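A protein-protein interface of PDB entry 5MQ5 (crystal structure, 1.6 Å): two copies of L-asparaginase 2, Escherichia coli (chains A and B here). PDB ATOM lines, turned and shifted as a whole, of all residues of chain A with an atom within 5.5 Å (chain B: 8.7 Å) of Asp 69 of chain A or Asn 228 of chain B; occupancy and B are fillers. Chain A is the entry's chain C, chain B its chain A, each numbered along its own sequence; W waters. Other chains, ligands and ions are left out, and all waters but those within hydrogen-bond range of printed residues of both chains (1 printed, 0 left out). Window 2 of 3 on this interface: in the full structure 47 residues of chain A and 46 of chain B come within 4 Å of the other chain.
The backbone carbonyl oxygen of Ala 227 of chain B lies within hydrogen-bond range of the guanidinium group of Arg 309 of chain A, at 3.2 Å. The backbone carbonyl oxygen (O) of Met 67 of chain A is in hydrogen-bond range of the backbone NH (N) of Asn 228 of chain B. N of Asp 69 of chain A sits close to ND2 of Asn 228 of chain B, at 2.8 Å.
The side-chain amide oxygen (OD1) of Asn 225 of chain B sits at hydrogen-bond distance from the backbone NH (N) of Tyr 256 of chain B (3.0 Å). The side-chain hydroxyl (OG) of Ser 230 of chain B lies within hydrogen-bond range of the backbone NH (N) of Leu 232 of chain B. The side-chain amide oxygen (OD1) of Asn 68 of chain A sits at hydrogen-bond distance from the backbone NH (N) of Asn 70 of chain A, 3.0 Å away. NH2 of Arg 309 of chain A lies within salt-bridge range of OD1 of Asp 69 of chain A (3.1 Å). The side-chain carboxylate of Asp 69 of chain A lies within hydrogen-bond range of the side-chain amide nitrogen of Gln 313 of chain A, 3.3 Å away. NE2 of Gln 313 of chain A lies close to NH2 of Arg 309 of chain A (3.2 Å).
Among the printed residues, pairs that only touch across the chains: Tyr 242 of chain A with Ser 230 of chain B (3.2 Å), Asn 68 of chain A with Asn 228 of chain B (3.3 Å), Arg 309 of chain A with Asn 228 of chain B (3.3 Å), Met 67 of chain A with Tyr 256 of chain B (3.4 Å), Met 67 of chain A with Ala 227 of chain B (3.4 Å), Arg 309 of chain A with Tyr 226 of chain B (3.5 Å) and Trp 72 of chain A with Ala 227 of chain B (3.5 Å).
Printed residues of chain B within 4 Å of Trp 72 of chain A: Ala 227 (3.5 Å). Printed residues of chain B within 4 Å of Arg 309 of chain A: Tyr 226 (3.5 Å), Ala 227 (3.2 Å) and Asn 228 (3.3 Å). Of the printed residues of chain A, Tyr 226 of chain B touches Arg 309 (3.5 Å). Asn 228 of chain B touches just these residues of chain A: Met 67 (3.0 Å), Asn 68 (3.3 Å), Asp 69 (2.8 Å) and Arg 309 (3.3 Å). Printed residues of chain A within 4 Å of Ser 230 of chain B: Tyr 242 (3.2 Å). Val 250 of chain B touches none of the printed residues of chain A. Of the printed residues of chain A, Tyr 256 of chain B touches Met 67 (3.4 Å). The nearest residue of chain A that does not touch Asn 228 of chain B is Asn 70 of chain A (4.8 Å).
Of the 14 printed residues of chain A, 6 touch a printed residue of chain B. Printed residues of chain B that touch a printed residue of chain A: Tyr 226, Ala 227, Asn 228, Ser 230 and Tyr 256. Among the printed residues, no Asp or Glu carboxylate lies within 4 Å of a Lys or Arg side-chain nitrogen of the other chain.
No position is printed for both chains.
Water W1 lies within hydrogen-bond range of OH of Tyr 256 of chain B (2.9 Å) and ND2 of Asn 68 of chain A (3.1 Å).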
ATOM      1  N   MET A  67     -15.213  -7.088   8.440  1.00  0.00           N
ATOM      2  CA  MET A  67     -14.482  -6.923   7.188  1.00  0.00           C
ATOM      3  C   MET A  67     -14.898  -5.629   6.484  1.00  0.00           C
ATOM      4  O   MET A  67     -16.023  -5.154   6.632  1.00  0.00           O
ATOM      5  CB  MET A  67     -14.748  -8.138   6.290  1.00  0.00           C
ATOM      6  CG  MET A  67     -13.889  -8.249   5.041  1.00  0.00           C
ATOM      7  SD  MET A  67     -12.109  -8.150   5.355  1.00  0.00           S
ATOM      8  CE  MET A  67     -11.831  -9.395   6.602  1.00  0.00           C
ATOM      9  N   ASN A  68     -13.986  -5.057   5.695  1.00  0.00           N
ATOM     10  CA  ASN A  68     -14.259  -3.737   5.127  1.00  0.00           C
ATOM     11  C   ASN A  68     -13.416  -3.499   3.879  1.00  0.00           C
ATOM     12  O   ASN A  68     -12.531  -4.289   3.540  1.00  0.00           O
ATOM     13  CB  ASN A  68     -13.996  -2.634   6.155  1.00  0.00           C
ATOM     14  CG  ASN A  68     -12.569  -2.663   6.663  1.00  0.00           C
ATOM     15  OD1 ASN A  68     -11.639  -2.313   5.939  1.00  0.00           O
ATOM     16  ND2 ASN A  68     -12.383  -3.127   7.898  1.00  0.00           N
ATOM     17  N   ASP A  69     -13.702  -2.367   3.215  1.00  0.00           N
ATOM     18  CA  ASP A  69     -13.044  -2.030   1.949  1.00  0.00           C
ATOM     19  C   ASP A  69     -11.533  -1.917   2.111  1.00  0.00           C
ATOM     20  O   ASP A  69     -10.771  -2.281   1.201  1.00  0.00           O
ATOM     21  CB  ASP A  69     -13.560  -0.693   1.410  1.00  0.00           C
ATOM     22  CG  ASP A  69     -14.995  -0.732   0.913  1.00  0.00           C
ATOM     23  OD1 ASP A  69     -15.659  -1.792   0.923  1.00  0.00           O
ATOM     24  OD2 ASP A  69     -15.449   0.362   0.514  1.00  0.00           O
ATOM     25  N   ASN A  70     -11.148  -1.387   3.132  1.00  0.00           N
ATOM     26  CA  ASN A  70      -9.725  -1.148   3.341  1.00  0.00           C
ATOM     27  C   ASN A  70      -8.945  -2.459   3.399  1.00  0.00           C
ATOM     28  O   ASN A  70      -7.837  -2.556   2.865  1.00  0.00           O
ATOM     29  CB  ASN A  70      -9.508  -0.342   4.629  1.00  0.00           C
ATOM     30  CG  ASN A  70      -9.961   1.116   4.515  1.00  0.00           C
ATOM     31  OD1 ASN A  70     -10.043   1.659   3.409  1.00  0.00           O
ATOM     32  ND2 ASN A  70     -10.236   1.755   5.643  1.00  0.00           N
ATOM     33  N   VAL A  71      -9.424  -3.445   4.094  1.00  0.00           N
ATOM     34  CA  VAL A  71      -8.746  -4.738   4.146  1.00  0.00           C
ATOM     35  C   VAL A  71      -8.749  -5.396   2.775  1.00  0.00           C
ATOM     36  O   VAL A  71      -7.760  -6.019   2.367  1.00  0.00           O
ATOM     37  CB  VAL A  71      -9.408  -5.641   5.198  1.00  0.00           C
ATOM     38  CG1 VAL A  71      -8.724  -7.006   5.233  1.00  0.00           C
ATOM     39  CG2 VAL A  71      -9.382  -4.975   6.563  1.00  0.00           C
ATOM     40  N   TRP A  72      -9.870  -5.301   2.058  1.00  0.00           N
ATOM     41  CA  TRP A  72      -9.931  -5.845   0.705  1.00  0.00           C
ATOM     42  C   TRP A  72      -8.847  -5.248  -0.175  1.00  0.00           C
ATOM     43  O   TRP A  72      -8.139  -5.969  -0.890  1.00  0.00           O
ATOM     44  CB  TRP A  72     -11.299  -5.575   0.094  1.00  0.00           C
ATOM     45  CG  TRP A  72     -12.385  -6.447   0.621  1.00  0.00           C
ATOM     46  CD1 TRP A  72     -12.269  -7.449   1.544  1.00  0.00           C
ATOM     47  CD2 TRP A  72     -13.762  -6.394   0.248  1.00  0.00           C
ATOM     48  NE1 TRP A  72     -13.503  -8.018   1.775  1.00  0.00           N
ATOM     49  CE2 TRP A  72     -14.436  -7.387   0.994  1.00  0.00           C
ATOM     50  CE3 TRP A  72     -14.497  -5.589  -0.637  1.00  0.00           C
ATOM     51  CZ2 TRP A  72     -15.810  -7.609   0.874  1.00  0.00           C
ATOM     52  CZ3 TRP A  72     -15.863  -5.812  -0.762  1.00  0.00           C
ATOM     53  CH2 TRP A  72     -16.504  -6.812  -0.005  1.00  0.00           C
ATOM     54  N   LEU A  73      -8.721  -3.920  -0.155  1.00  0.00           N
ATOM     55  CA  LEU A  73      -7.702  -3.268  -0.970  1.00  0.00           C
ATOM     56  C   LEU A  73      -6.301  -3.694  -0.547  1.00  0.00           C
ATOM     57  O   LEU A  73      -5.436  -3.926  -1.396  1.00  0.00           O
ATOM     58  CB  LEU A  73      -7.855  -1.748  -0.887  1.00  0.00           C
ATOM     59  CG  LEU A  73      -9.091  -1.161  -1.582  1.00  0.00           C
ATOM     60  CD1 LEU A  73      -9.313   0.294  -1.183  1.00  0.00           C
ATOM     61  CD2 LEU A  73      -8.942  -1.293  -3.092  1.00  0.00           C
ATOM     62  N   THR A  74      -6.068  -3.813   0.763  1.00  0.00           N
ATOM     63  CA  THR A  74      -4.773  -4.273   1.257  1.00  0.00           C
ATOM     64  C   THR A  74      -4.438  -5.664   0.733  1.00  0.00           C
ATOM     65  O   THR A  74      -3.302  -5.910   0.299  1.00  0.00           O
ATOM     66  CB  THR A  74      -4.759  -4.265   2.784  1.00  0.00           C
ATOM     67  OG1 THR A  74      -4.947  -2.923   3.260  1.00  0.00           O
ATOM     68  CG2 THR A  74      -3.439  -4.822   3.314  1.00  0.00           C
ATOM     69  N   GLU A 216      -9.917   3.915  -1.932  1.00  0.00           N
ATOM     70  CA  GLU A 216     -11.270   3.708  -1.442  1.00  0.00           C
ATOM     71  C   GLU A 216     -12.075   3.103  -2.576  1.00  0.00           C
ATOM     72  O   GLU A 216     -11.636   3.071  -3.728  1.00  0.00           O
ATOM     73  CB  GLU A 216     -11.898   5.018  -0.960  1.00  0.00           C
ATOM     74  CG  GLU A 216     -12.163   5.999  -2.084  1.00  0.00           C
ATOM     75  CD  GLU A 216     -12.878   7.249  -1.611  1.00  0.00           C
ATOM     76  OE1 GLU A 216     -12.293   8.007  -0.802  1.00  0.00           O
ATOM     77  OE2 GLU A 216     -14.027   7.467  -2.046  1.00  0.00           O
ATOM     78  N   LEU A 217     -13.256   2.606  -2.231  1.00  0.00           N
ATOM     79  CA  LEU A 217     -14.156   2.030  -3.210  1.00  0.00           C
ATOM     80  C   LEU A 217     -15.483   2.780  -3.220  1.00  0.00           C
ATOM     81  O   LEU A 217     -15.889   3.348  -2.198  1.00  0.00           O
ATOM     82  CB  LEU A 217     -14.412   0.546  -2.921  1.00  0.00           C
ATOM     83  CG  LEU A 217     -13.217  -0.402  -3.059  1.00  0.00           C
ATOM     84  CD1 LEU A 217     -13.583  -1.793  -2.556  1.00  0.00           C
ATOM     85  CD2 LEU A 217     -12.746  -0.473  -4.489  1.00  0.00           C
ATOM     86  N   PRO A 218     -16.164   2.817  -4.366  1.00  0.00           N
ATOM     87  CA  PRO A 218     -17.486   3.448  -4.431  1.00  0.00           C
ATOM     88  C   PRO A 218     -18.417   2.912  -3.352  1.00  0.00           C
ATOM     89  O   PRO A 218     -18.335   1.746  -2.946  1.00  0.00           O
ATOM     90  CB  PRO A 218     -17.981   3.084  -5.836  1.00  0.00           C
ATOM     91  CG  PRO A 218     -16.704   2.908  -6.630  1.00  0.00           C
ATOM     92  CD  PRO A 218     -15.741   2.274  -5.671  1.00  0.00           C
ATOM     93  N   TYR A 242     -25.042   7.709  -1.861  1.00  0.00           N
ATOM     94  CA  TYR A 242     -24.442   6.428  -2.203  1.00  0.00           C
ATOM     95  C   TYR A 242     -24.325   6.289  -3.717  1.00  0.00           C
ATOM     96  O   TYR A 242     -25.200   6.726  -4.466  1.00  0.00           O
ATOM     97  CB  TYR A 242     -25.268   5.280  -1.600  1.00  0.00           C
ATOM     98  CG  TYR A 242     -24.607   4.778  -0.352  1.00  0.00           C
ATOM     99  CD1 TYR A 242     -24.355   5.642   0.705  1.00  0.00           C
ATOM    100  CD2 TYR A 242     -24.162   3.464  -0.252  1.00  0.00           C
ATOM    101  CE1 TYR A 242     -23.708   5.201   1.843  1.00  0.00           C
ATOM    102  CE2 TYR A 242     -23.508   3.020   0.873  1.00  0.00           C
ATOM    103  CZ  TYR A 242     -23.287   3.889   1.918  1.00  0.00           C
ATOM    104  OH  TYR A 242     -22.630   3.441   3.033  1.00  0.00           O
ATOM    105  N   ARG A 309     -23.046  -6.520  -4.433  1.00  0.00           N
ATOM    106  CA  ARG A 309     -22.377  -5.308  -3.972  1.00  0.00           C
ATOM    107  C   ARG A 309     -20.918  -5.274  -4.414  1.00  0.00           C
ATOM    108  O   ARG A 309     -20.433  -4.245  -4.897  1.00  0.00           O
ATOM    109  CB  ARG A 309     -22.467  -5.195  -2.451  1.00  0.00           C
ATOM    110  CG  ARG A 309     -21.519  -4.127  -1.892  1.00  0.00           C
ATOM    111  CD  ARG A 309     -21.673  -3.923  -0.377  1.00  0.00           C
ATOM    112  NE  ARG A 309     -20.770  -2.860   0.074  1.00  0.00           N
ATOM    113  CZ  ARG A 309     -19.518  -3.075   0.467  1.00  0.00           C
ATOM    114  NH1 ARG A 309     -19.033  -4.306   0.470  1.00  0.00           N
ATOM    115  NH2 ARG A 309     -18.746  -2.055   0.850  1.00  0.00           N
ATOM    116  N   GLN A 313     -19.558  -2.282  -6.824  1.00  0.00           N
ATOM    117  CA  GLN A 313     -18.521  -1.334  -6.419  1.00  0.00           C
ATOM    118  C   GLN A 313     -17.447  -1.251  -7.488  1.00  0.00           C
ATOM    119  O   GLN A 313     -17.024  -0.161  -7.890  1.00  0.00           O
ATOM    120  CB  GLN A 313     -17.878  -1.758  -5.103  1.00  0.00           C
ATOM    121  CG  GLN A 313     -18.662  -1.524  -3.832  1.00  0.00           C
ATOM    122  CD  GLN A 313     -17.802  -1.849  -2.626  1.00  0.00           C
ATOM    123  OE1 GLN A 313     -17.415  -2.994  -2.435  1.00  0.00           O
ATOM    124  NE2 GLN A 313     -17.452  -0.830  -1.841  1.00  0.00           N
ATOM    125  N   TYR B 224     -29.765  -5.250   6.760  1.00  0.00           N
ATOM    126  CA  TYR B 224     -28.854  -6.264   6.239  1.00  0.00           C
ATOM    127  C   TYR B 224     -27.420  -6.002   6.693  1.00  0.00           C
ATOM    128  O   TYR B 224     -26.984  -4.850   6.777  1.00  0.00           O
ATOM    129  CB  TYR B 224     -28.910  -6.275   4.709  1.00  0.00           C
ATOM    130  CG  TYR B 224     -28.599  -7.597   4.033  1.00  0.00           C
ATOM    131  CD1 TYR B 224     -29.513  -8.647   4.066  1.00  0.00           C
ATOM    132  CD2 TYR B 224     -27.408  -7.777   3.318  1.00  0.00           C
ATOM    133  CE1 TYR B 224     -29.248  -9.854   3.429  1.00  0.00           C
ATOM    134  CE2 TYR B 224     -27.128  -8.990   2.662  1.00  0.00           C
ATOM    135  CZ  TYR B 224     -28.063 -10.022   2.727  1.00  0.00           C
ATOM    136  OH  TYR B 224     -27.843 -11.229   2.103  1.00  0.00           O
ATOM    137  N   ASN B 225     -26.676  -7.077   6.950  1.00  0.00           N
ATOM    138  CA  ASN B 225     -25.265  -6.981   7.299  1.00  0.00           C
ATOM    139  C   ASN B 225     -24.402  -7.590   6.201  1.00  0.00           C
ATOM    140  O   ASN B 225     -24.797  -8.563   5.544  1.00  0.00           O
ATOM    141  CB  ASN B 225     -24.956  -7.691   8.622  1.00  0.00           C
ATOM    142  CG  ASN B 225     -25.511  -6.950   9.828  1.00  0.00           C
ATOM    143  OD1 ASN B 225     -24.804  -6.170  10.469  1.00  0.00           O
ATOM    144  ND2 ASN B 225     -26.777  -7.208  10.157  1.00  0.00           N
ATOM    145  N   TYR B 226     -23.212  -7.010   6.029  1.00  0.00           N
ATOM    146  CA  TYR B 226     -22.257  -7.349   4.978  1.00  0.00           C
ATOM    147  C   TYR B 226     -20.985  -6.569   5.292  1.00  0.00           C
ATOM    148  O   TYR B 226     -20.967  -5.742   6.203  1.00  0.00           O
ATOM    149  CB  TYR B 226     -22.817  -6.996   3.598  1.00  0.00           C
ATOM    150  CG  TYR B 226     -23.367  -5.579   3.514  1.00  0.00           C
ATOM    151  CD1 TYR B 226     -24.616  -5.263   4.037  1.00  0.00           C
ATOM    152  CD2 TYR B 226     -22.631  -4.569   2.911  1.00  0.00           C
ATOM    153  CE1 TYR B 226     -25.115  -3.982   3.977  1.00  0.00           C
ATOM    154  CE2 TYR B 226     -23.127  -3.280   2.828  1.00  0.00           C
ATOM    155  CZ  TYR B 226     -24.379  -2.996   3.369  1.00  0.00           C
ATOM    156  OH  TYR B 226     -24.895  -1.724   3.309  1.00  0.00           O
ATOM    157  N   ALA B 227     -19.919  -6.851   4.550  1.00  0.00           N
ATOM    158  CA  ALA B 227     -18.668  -6.117   4.743  1.00  0.00           C
ATOM    159  C   ALA B 227     -18.908  -4.620   4.541  1.00  0.00           C
ATOM    160  O   ALA B 227     -19.598  -4.216   3.599  1.00  0.00           O
ATOM    161  CB  ALA B 227     -17.600  -6.618   3.769  1.00  0.00           C
ATOM    162  N   ASN B 228     -18.352  -3.796   5.433  1.00  0.00           N
ATOM    163  CA  ASN B 228     -18.451  -2.356   5.311  1.00  0.00           C
ATOM    164  C   ASN B 228     -19.869  -1.820   5.368  1.00  0.00           C
ATOM    165  O   ASN B 228     -20.146  -0.804   4.867  1.00  0.00           O
ATOM    166  CB  ASN B 228     -17.763  -1.910   4.009  1.00  0.00           C
ATOM    167  CG  ASN B 228     -17.016  -0.595   4.147  1.00  0.00           C
ATOM    168  OD1 ASN B 228     -17.618   0.420   4.228  1.00  0.00           O
ATOM    169  ND2 ASN B 228     -15.746  -0.649   4.184  1.00  0.00           N
ATOM    170  N   ALA B 229     -20.728  -2.509   6.081  1.00  0.00           N
ATOM    171  CA  ALA B 229     -22.140  -2.143   6.085  1.00  0.00           C
ATOM    172  C   ALA B 229     -22.375  -0.766   6.693  1.00  0.00           C
ATOM    173  O   ALA B 229     -21.848  -0.431   7.756  1.00  0.00           O
ATOM    174  CB  ALA B 229     -22.954  -3.186   6.855  1.00  0.00           C
ATOM    175  N   SER B 230     -23.216   0.016   6.023  1.00  0.00           N
ATOM    176  CA  SER B 230     -23.594   1.328   6.535  1.00  0.00           C
ATOM    177  C   SER B 230     -24.523   1.189   7.735  1.00  0.00           C
ATOM    178  O   SER B 230     -25.396   0.312   7.776  1.00  0.00           O
ATOM    179  CB  SER B 230     -24.290   2.140   5.445  1.00  0.00           C
ATOM    180  OG  SER B 230     -24.800   3.363   5.961  1.00  0.00           O
ATOM    181  N   ASP B 231     -24.358   2.081   8.707  1.00  0.00           N
ATOM    182  CA  ASP B 231     -25.321   2.143   9.799  1.00  0.00           C
ATOM    183  C   ASP B 231     -26.549   2.990   9.472  1.00  0.00           C
ATOM    184  O   ASP B 231     -27.441   3.114  10.322  1.00  0.00           O
ATOM    185  CB  ASP B 231     -24.653   2.664  11.083  1.00  0.00           C
ATOM    186  CG  ASP B 231     -24.121   4.088  10.958  1.00  0.00           C
ATOM    187  OD1 ASP B 231     -24.411   4.801   9.965  1.00  0.00           O
ATOM    188  OD2 ASP B 231     -23.395   4.498  11.886  1.00  0.00           O
ATOM    189  N   LEU B 232     -26.640   3.550   8.269  1.00  0.00           N
ATOM    190  CA  LEU B 232     -27.708   4.494   7.954  1.00  0.00           C
ATOM    191  C   LEU B 232     -29.087   3.842   7.914  1.00  0.00           C
ATOM    192  O   LEU B 232     -30.057   4.450   8.392  1.00  0.00           O
ATOM    193  CB  LEU B 232     -27.419   5.205   6.633  1.00  0.00           C
ATOM    194  CG  LEU B 232     -26.238   6.170   6.709  1.00  0.00           C
ATOM    195  CD1 LEU B 232     -25.849   6.603   5.310  1.00  0.00           C
ATOM    196  CD2 LEU B 232     -26.568   7.369   7.597  1.00  0.00           C
ATOM    197  N   VAL B 250     -24.629 -11.612   9.653  1.00  0.00           N
ATOM    198  CA  VAL B 250     -23.747 -12.513   8.919  1.00  0.00           C
ATOM    199  C   VAL B 250     -23.454 -13.707   9.817  1.00  0.00           C
ATOM    200  O   VAL B 250     -23.366 -13.587  11.041  1.00  0.00           O
ATOM    201  CB  VAL B 250     -22.454 -11.806   8.445  1.00  0.00           C
ATOM    202  CG1 VAL B 250     -22.776 -10.714   7.427  1.00  0.00           C
ATOM    203  CG2 VAL B 250     -21.659 -11.228   9.624  1.00  0.00           C
ATOM    204  N   TYR B 256     -22.117  -6.161  11.703  1.00  0.00           N
ATOM    205  CA  TYR B 256     -21.044  -5.227  11.391  1.00  0.00           C
ATOM    206  C   TYR B 256     -20.959  -4.169  12.490  1.00  0.00           C
ATOM    207  O   TYR B 256     -21.983  -3.703  12.994  1.00  0.00           O
ATOM    208  CB  TYR B 256     -21.295  -4.579  10.035  1.00  0.00           C
ATOM    209  CG  TYR B 256     -20.171  -3.670   9.626  1.00  0.00           C
ATOM    210  CD1 TYR B 256     -18.985  -4.197   9.131  1.00  0.00           C
ATOM    211  CD2 TYR B 256     -20.278  -2.289   9.773  1.00  0.00           C
ATOM    212  CE1 TYR B 256     -17.927  -3.370   8.761  1.00  0.00           C
ATOM    213  CE2 TYR B 256     -19.228  -1.451   9.413  1.00  0.00           C
ATOM    214  CZ  TYR B 256     -18.058  -2.003   8.907  1.00  0.00           C
ATOM    215  OH  TYR B 256     -16.999  -1.205   8.537  1.00  0.00           O
ATOM    216  N   LYS B 257     -19.725  -3.795  12.859  1.00  0.00           N
ATOM    217  CA  LYS B 257     -19.500  -2.953  14.043  1.00  0.00           C
ATOM    218  C   LYS B 257     -20.399  -1.716  14.077  1.00  0.00           C
ATOM    219  O   LYS B 257     -21.005  -1.411  15.112  1.00  0.00           O
ATOM    220  CB  LYS B 257     -18.026  -2.540  14.120  1.00  0.00           C
ATOM    221  CG  LYS B 257     -17.491  -1.884  12.857  1.00  0.00           C
ATOM    222  CD  LYS B 257     -16.031  -1.470  13.003  1.00  0.00           C
ATOM    223  CE  LYS B 257     -15.820  -0.020  12.572  1.00  0.00           C
ATOM    224  NZ  LYS B 257     -16.563   0.950  13.432  1.00  0.00           N
ATOM    225  N   SER B 258     -20.495  -0.981  12.962  1.00  0.00           N
ATOM    226  CA  SER B 258     -21.324   0.227  12.939  1.00  0.00           C
ATOM    227  C   SER B 258     -22.789  -0.103  13.199  1.00  0.00           C
ATOM    228  O   SER B 258     -23.484   0.621  13.928  1.00  0.00           O
ATOM    229  CB  SER B 258     -21.178   0.937  11.593  1.00  0.00           C
ATOM    230  OG  SER B 258     -19.829   1.278  11.365  1.00  0.00           O
ATOM    231  N   VAL B 259     -23.271  -1.206  12.617  1.00  0.00           N
ATOM    232  CA  VAL B 259     -24.648  -1.632  12.848  1.00  0.00           C
ATOM    233  C   VAL B 259     -24.835  -2.084  14.293  1.00  0.00           C
ATOM    234  O   VAL B 259     -25.839  -1.759  14.933  1.00  0.00           O
ATOM    235  CB  VAL B 259     -25.021  -2.746  11.850  1.00  0.00           C
ATOM    236  CG1 VAL B 259     -26.462  -3.229  12.077  1.00  0.00           C
ATOM    237  CG2 VAL B 259     -24.822  -2.235  10.415  1.00  0.00           C
ATOM    238  N   ARG B 278     -28.774 -13.547   7.584  1.00  0.00           N
ATOM    239  CA  ARG B 278     -28.914 -13.684   6.131  1.00  0.00           C
ATOM    240  C   ARG B 278     -28.597 -15.090   5.636  1.00  0.00           C
ATOM    241  O   ARG B 278     -28.895 -15.408   4.477  1.00  0.00           O
ATOM    242  CB  ARG B 278     -27.981 -12.708   5.416  1.00  0.00           C
ATOM    243  CG  ARG B 278     -26.538 -13.189   5.367  1.00  0.00           C
ATOM    244  CD  ARG B 278     -25.608 -12.076   4.853  1.00  0.00           C
ATOM    245  NE  ARG B 278     -24.279 -12.615   4.599  1.00  0.00           N
ATOM    246  CZ  ARG B 278     -23.254 -11.911   4.116  1.00  0.00           C
ATOM    247  NH1 ARG B 278     -23.377 -10.610   3.883  1.00  0.00           N
ATOM    248  NH2 ARG B 278     -22.096 -12.520   3.873  1.00  0.00           N
HETATM  249  O   HOH W   1     -14.639  -2.258   9.875  1.00  0.00           O
